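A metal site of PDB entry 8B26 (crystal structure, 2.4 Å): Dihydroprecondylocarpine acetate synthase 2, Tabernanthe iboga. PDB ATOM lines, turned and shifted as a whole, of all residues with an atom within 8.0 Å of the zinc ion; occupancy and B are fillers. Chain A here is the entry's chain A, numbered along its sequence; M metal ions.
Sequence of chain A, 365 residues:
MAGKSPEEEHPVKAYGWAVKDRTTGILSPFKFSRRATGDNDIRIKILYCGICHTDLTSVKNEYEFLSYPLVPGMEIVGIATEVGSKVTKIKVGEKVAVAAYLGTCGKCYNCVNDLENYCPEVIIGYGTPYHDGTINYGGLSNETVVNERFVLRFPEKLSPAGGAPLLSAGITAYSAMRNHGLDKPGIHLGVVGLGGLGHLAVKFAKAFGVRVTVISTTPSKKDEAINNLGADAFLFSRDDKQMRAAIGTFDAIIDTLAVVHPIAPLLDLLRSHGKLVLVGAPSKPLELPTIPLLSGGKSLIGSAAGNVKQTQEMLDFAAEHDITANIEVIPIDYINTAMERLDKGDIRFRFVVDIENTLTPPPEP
SG of Cys 108 lies close to N of Asn 110 (3.6 Å).
The backbone NH (N) of Gly 106 sits close to the side-chain sulfur (SG) of Cys 111.
The side-chain sulfur (SG) of Cys 111 sits close to the side-chain hydroxyl (OG1) of Thr 104 (3.5 Å).
O of Cys 111 sits at hydrogen-bond distance from NH2 of Arg 149 (2.8 Å).
The side-chain sulfur (SG) of Cys 119 sits close to the backbone NH (N) of Glu 121 (3.2 Å).
SG of Cys 105 lies close to N of Lys 107, 3.0 Å away.
Merely in contact with the zinc ion: Gly 106.
Within 4 Å of the zinc ion: Cys 105, Gly 106, Cys 108, Cys 111 and Cys 119.
The nearest printed residue that does not touch the zinc ion is Lys 107 (4.3 Å).
SG of Cys 108 binds the zinc ion.
The zinc ion is bound by SG of Cys 111.
The zinc ion is bound by SG of Cys 119, at 2.3 Å.
SG of Cys 105 binds the zinc ion, 2.3 Å away.
The zinc ion has four donor atoms within binding distance.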
ATOM      1  N   GLY A 103      -1.839 -24.952 -17.325  1.00  0.00           N
ATOM      2  CA  GLY A 103      -1.074 -23.913 -16.660  1.00  0.00           C
ATOM      3  C   GLY A 103       0.292 -23.746 -17.275  1.00  0.00           C
ATOM      4  O   GLY A 103       0.736 -24.556 -18.099  1.00  0.00           O
ATOM      5  N   THR A 104       0.965 -22.681 -16.842  1.00  0.00           N
ATOM      6  CA  THR A 104       2.284 -22.304 -17.350  1.00  0.00           C
ATOM      7  C   THR A 104       3.086 -21.679 -16.209  1.00  0.00           C
ATOM      8  O   THR A 104       2.541 -21.342 -15.157  1.00  0.00           O
ATOM      9  CB  THR A 104       2.188 -21.327 -18.532  1.00  0.00           C
ATOM     10  OG1 THR A 104       1.308 -20.244 -18.194  1.00  0.00           O
ATOM     11  CG2 THR A 104       1.675 -22.024 -19.783  1.00  0.00           C
ATOM     12  N   CYS A 105       4.402 -21.579 -16.425  1.00  0.00           N
ATOM     13  CA  CYS A 105       5.265 -20.944 -15.433  1.00  0.00           C
ATOM     14  C   CYS A 105       4.783 -19.544 -15.070  1.00  0.00           C
ATOM     15  O   CYS A 105       4.803 -19.152 -13.901  1.00  0.00           O
ATOM     16  CB  CYS A 105       6.706 -20.866 -15.957  1.00  0.00           C
ATOM     17  SG  CYS A 105       7.045 -19.388 -16.933  1.00  0.00           S
ATOM     18  N   GLY A 106       4.338 -18.778 -16.063  1.00  0.00           N
ATOM     19  CA  GLY A 106       3.815 -17.447 -15.827  1.00  0.00           C
ATOM     20  C   GLY A 106       4.849 -16.342 -15.760  1.00  0.00           C
ATOM     21  O   GLY A 106       4.480 -15.186 -15.508  1.00  0.00           O
ATOM     22  N   LYS A 107       6.132 -16.636 -15.996  1.00  0.00           N
ATOM     23  CA  LYS A 107       7.176 -15.631 -15.898  1.00  0.00           C
ATOM     24  C   LYS A 107       8.110 -15.557 -17.102  1.00  0.00           C
ATOM     25  O   LYS A 107       8.962 -14.662 -17.133  1.00  0.00           O
ATOM     26  CB  LYS A 107       8.033 -15.878 -14.642  1.00  0.00           C
ATOM     27  CG  LYS A 107       8.873 -17.157 -14.717  1.00  0.00           C
ATOM     28  CD  LYS A 107      10.346 -16.873 -15.029  1.00  0.00           C
ATOM     29  CE  LYS A 107      11.103 -18.147 -15.386  1.00  0.00           C
ATOM     30  NZ  LYS A 107      12.253 -17.875 -16.297  1.00  0.00           N
ATOM     31  N   CYS A 108       7.973 -16.439 -18.088  1.00  0.00           N
ATOM     32  CA  CYS A 108       8.798 -16.333 -19.280  1.00  0.00           C
ATOM     33  C   CYS A 108       8.186 -15.331 -20.260  1.00  0.00           C
ATOM     34  O   CYS A 108       7.093 -14.800 -20.059  1.00  0.00           O
ATOM     35  CB  CYS A 108       8.977 -17.705 -19.933  1.00  0.00           C
ATOM     36  SG  CYS A 108       7.501 -18.382 -20.701  1.00  0.00           S
ATOM     37  N   TYR A 109       8.938 -15.052 -21.332  1.00  0.00           N
ATOM     38  CA  TYR A 109       8.479 -14.147 -22.377  1.00  0.00           C
ATOM     39  C   TYR A 109       7.150 -14.610 -22.963  1.00  0.00           C
ATOM     40  O   TYR A 109       6.217 -13.814 -23.136  1.00  0.00           O
ATOM     41  CB  TYR A 109       9.532 -14.026 -23.474  1.00  0.00           C
ATOM     42  CG  TYR A 109       9.095 -13.216 -24.692  1.00  0.00           C
ATOM     43  CD1 TYR A 109       8.424 -13.822 -25.745  1.00  0.00           C
ATOM     44  CD2 TYR A 109       9.379 -11.856 -24.783  1.00  0.00           C
ATOM     45  CE1 TYR A 109       8.022 -13.091 -26.852  1.00  0.00           C
ATOM     46  CE2 TYR A 109       8.986 -11.123 -25.887  1.00  0.00           C
ATOM     47  CZ  TYR A 109       8.303 -11.752 -26.913  1.00  0.00           C
ATOM     48  OH  TYR A 109       7.911 -11.018 -28.017  1.00  0.00           O
ATOM     49  N   ASN A 110       7.067 -15.894 -23.313  1.00  0.00           N
ATOM     50  CA  ASN A 110       5.851 -16.430 -23.922  1.00  0.00           C
ATOM     51  C   ASN A 110       4.634 -16.181 -23.036  1.00  0.00           C
ATOM     52  O   ASN A 110       3.584 -15.723 -23.520  1.00  0.00           O
ATOM     53  CB  ASN A 110       6.022 -17.922 -24.198  1.00  0.00           C
ATOM     54  CG  ASN A 110       7.196 -18.206 -25.127  1.00  0.00           C
ATOM     55  OD1 ASN A 110       7.252 -17.703 -26.250  1.00  0.00           O
ATOM     56  ND2 ASN A 110       8.151 -19.002 -24.648  1.00  0.00           N
ATOM     57  N   CYS A 111       4.739 -16.476 -21.740  1.00  0.00           N
ATOM     58  CA  CYS A 111       3.602 -16.329 -20.845  1.00  0.00           C
ATOM     59  C   CYS A 111       3.133 -14.876 -20.767  1.00  0.00           C
ATOM     60  O   CYS A 111       1.931 -14.595 -20.841  1.00  0.00           O
ATOM     61  CB  CYS A 111       3.968 -16.838 -19.451  1.00  0.00           C
ATOM     62  SG  CYS A 111       4.160 -18.616 -19.324  1.00  0.00           S
ATOM     63  N   VAL A 112       4.075 -13.938 -20.627  1.00  0.00           N
ATOM     64  CA  VAL A 112       3.691 -12.547 -20.371  1.00  0.00           C
ATOM     65  C   VAL A 112       3.155 -11.849 -21.620  1.00  0.00           C
ATOM     66  O   VAL A 112       2.447 -10.844 -21.506  1.00  0.00           O
ATOM     67  CB  VAL A 112       4.869 -11.732 -19.796  1.00  0.00           C
ATOM     68  CG1 VAL A 112       5.197 -12.209 -18.380  1.00  0.00           C
ATOM     69  CG2 VAL A 112       6.086 -11.816 -20.698  1.00  0.00           C
ATOM     70  N   LEU A 115       1.538 -15.738 -25.454  1.00  0.00           N
ATOM     71  CA  LEU A 115       1.944 -16.850 -26.297  1.00  0.00           C
ATOM     72  C   LEU A 115       2.268 -18.059 -25.422  1.00  0.00           C
ATOM     73  O   LEU A 115       3.256 -18.765 -25.647  1.00  0.00           O
ATOM     74  CB  LEU A 115       3.133 -16.474 -27.183  1.00  0.00           C
ATOM     75  CG  LEU A 115       3.134 -15.046 -27.713  1.00  0.00           C
ATOM     76  CD1 LEU A 115       4.466 -14.714 -28.375  1.00  0.00           C
ATOM     77  CD2 LEU A 115       1.985 -14.823 -28.677  1.00  0.00           C
ATOM     78  N   GLU A 116       1.421 -18.306 -24.427  1.00  0.00           N
ATOM     79  CA  GLU A 116       1.763 -19.177 -23.310  1.00  0.00           C
ATOM     80  C   GLU A 116       1.788 -20.651 -23.697  1.00  0.00           C
ATOM     81  O   GLU A 116       2.392 -21.448 -22.972  1.00  0.00           O
ATOM     82  CB  GLU A 116       0.781 -18.965 -22.152  1.00  0.00           C
ATOM     83  CG  GLU A 116      -0.652 -19.341 -22.495  1.00  0.00           C
ATOM     84  CD  GLU A 116      -1.385 -18.248 -23.258  1.00  0.00           C
ATOM     85  OE1 GLU A 116      -0.752 -17.218 -23.563  1.00  0.00           O
ATOM     86  OE2 GLU A 116      -2.576 -18.421 -23.559  1.00  0.00           O
ATOM     87  N   ASN A 117       1.121 -21.050 -24.784  1.00  0.00           N
ATOM     88  CA  ASN A 117       1.139 -22.454 -25.182  1.00  0.00           C
ATOM     89  C   ASN A 117       2.540 -22.929 -25.536  1.00  0.00           C
ATOM     90  O   ASN A 117       2.792 -24.135 -25.511  1.00  0.00           O
ATOM     91  CB  ASN A 117       0.192 -22.685 -26.362  1.00  0.00           C
ATOM     92  CG  ASN A 117       0.518 -21.811 -27.555  1.00  0.00           C
ATOM     93  OD1 ASN A 117       0.662 -20.594 -27.429  1.00  0.00           O
ATOM     94  ND2 ASN A 117       0.646 -22.423 -28.720  1.00  0.00           N
ATOM     95  N   TYR A 118       3.452 -22.010 -25.840  1.00  0.00           N
ATOM     96  CA  TYR A 118       4.846 -22.338 -26.130  1.00  0.00           C
ATOM     97  C   TYR A 118       5.743 -22.202 -24.904  1.00  0.00           C
ATOM     98  O   TYR A 118       6.964 -22.260 -25.046  1.00  0.00           O
ATOM     99  CB  TYR A 118       5.348 -21.478 -27.285  1.00  0.00           C
ATOM    100  CG  TYR A 118       4.747 -21.879 -28.603  1.00  0.00           C
ATOM    101  CD1 TYR A 118       5.132 -23.059 -29.225  1.00  0.00           C
ATOM    102  CD2 TYR A 118       3.762 -21.108 -29.215  1.00  0.00           C
ATOM    103  CE1 TYR A 118       4.582 -23.452 -30.426  1.00  0.00           C
ATOM    104  CE2 TYR A 118       3.212 -21.491 -30.426  1.00  0.00           C
ATOM    105  CZ  TYR A 118       3.619 -22.664 -31.021  1.00  0.00           C
ATOM    106  OH  TYR A 118       3.069 -23.057 -32.221  1.00  0.00           O
ATOM    107  N   CYS A 119       5.169 -22.003 -23.728  1.00  0.00           N
ATOM    108  CA  CYS A 119       5.966 -21.925 -22.510  1.00  0.00           C
ATOM    109  C   CYS A 119       6.758 -23.216 -22.328  1.00  0.00           C
ATOM    110  O   CYS A 119       6.222 -24.317 -22.559  1.00  0.00           O
ATOM    111  CB  CYS A 119       5.083 -21.673 -21.283  1.00  0.00           C
ATOM    112  SG  CYS A 119       5.957 -21.817 -19.698  1.00  0.00           S
ATOM    113  N   PRO A 120       8.027 -23.142 -21.935  1.00  0.00           N
ATOM    114  CA  PRO A 120       8.800 -24.361 -21.684  1.00  0.00           C
ATOM    115  C   PRO A 120       8.211 -25.238 -20.585  1.00  0.00           C
ATOM    116  O   PRO A 120       8.425 -26.457 -20.602  1.00  0.00           O
ATOM    117  CB  PRO A 120      10.186 -23.830 -21.288  1.00  0.00           C
ATOM    118  CG  PRO A 120      10.262 -22.469 -21.903  1.00  0.00           C
ATOM    119  CD  PRO A 120       8.863 -21.923 -21.816  1.00  0.00           C
ATOM    120  N   GLU A 121       7.485 -24.655 -19.637  1.00  0.00           N
ATOM    121  CA  GLU A 121       6.949 -25.381 -18.498  1.00  0.00           C
ATOM    122  C   GLU A 121       5.438 -25.495 -18.564  1.00  0.00           C
ATOM    123  O   GLU A 121       4.741 -25.420 -17.550  1.00  0.00           O
ATOM    124  CB  GLU A 121       7.365 -24.708 -17.181  1.00  0.00           C
ATOM    125  CG  GLU A 121       8.757 -25.083 -16.695  1.00  0.00           C
ATOM    126  CD  GLU A 121       9.307 -24.077 -15.695  1.00  0.00           C
ATOM    127  OE1 GLU A 121       8.545 -23.662 -14.793  1.00  0.00           O
ATOM    128  OE2 GLU A 121      10.490 -23.719 -15.816  1.00  0.00           O
ATOM    129  N   VAL A 122       4.911 -25.696 -19.773  1.00  0.00           N
ATOM    130  CA  VAL A 122       3.465 -25.787 -19.946  1.00  0.00           C
ATOM    131  C   VAL A 122       2.968 -27.088 -19.351  1.00  0.00           C
ATOM    132  O   VAL A 122       3.581 -28.153 -19.524  1.00  0.00           O
ATOM    133  CB  VAL A 122       3.084 -25.650 -21.437  1.00  0.00           C
ATOM    134  CG1 VAL A 122       3.648 -26.810 -22.259  1.00  0.00           C
ATOM    135  CG2 VAL A 122       1.574 -25.570 -21.591  1.00  0.00           C
ATOM    136  N   ARG A 149      -7.597 -18.258 -16.543  1.00  0.00           N
ATOM    137  CA  ARG A 149      -6.845 -17.913 -17.758  1.00  0.00           C
ATOM    138  C   ARG A 149      -7.032 -18.969 -18.846  1.00  0.00           C
ATOM    139  O   ARG A 149      -7.026 -18.639 -20.038  1.00  0.00           O
ATOM    140  CB  ARG A 149      -5.366 -17.743 -17.440  1.00  0.00           C
ATOM    141  CG  ARG A 149      -4.595 -16.949 -18.491  1.00  0.00           C
ATOM    142  CD  ARG A 149      -3.097 -17.223 -18.440  1.00  0.00           C
ATOM    143  NE  ARG A 149      -2.403 -16.610 -19.570  1.00  0.00           N
ATOM    144  CZ  ARG A 149      -1.152 -16.184 -19.545  1.00  0.00           C
ATOM    145  NH1 ARG A 149      -0.404 -16.303 -18.450  1.00  0.00           N
ATOM    146  NH2 ARG A 149      -0.624 -15.635 -20.630  1.00  0.00           N
HETATM  147 ZN    ZN M   1       6.277 -19.576 -19.131  1.00  0.00          ZN
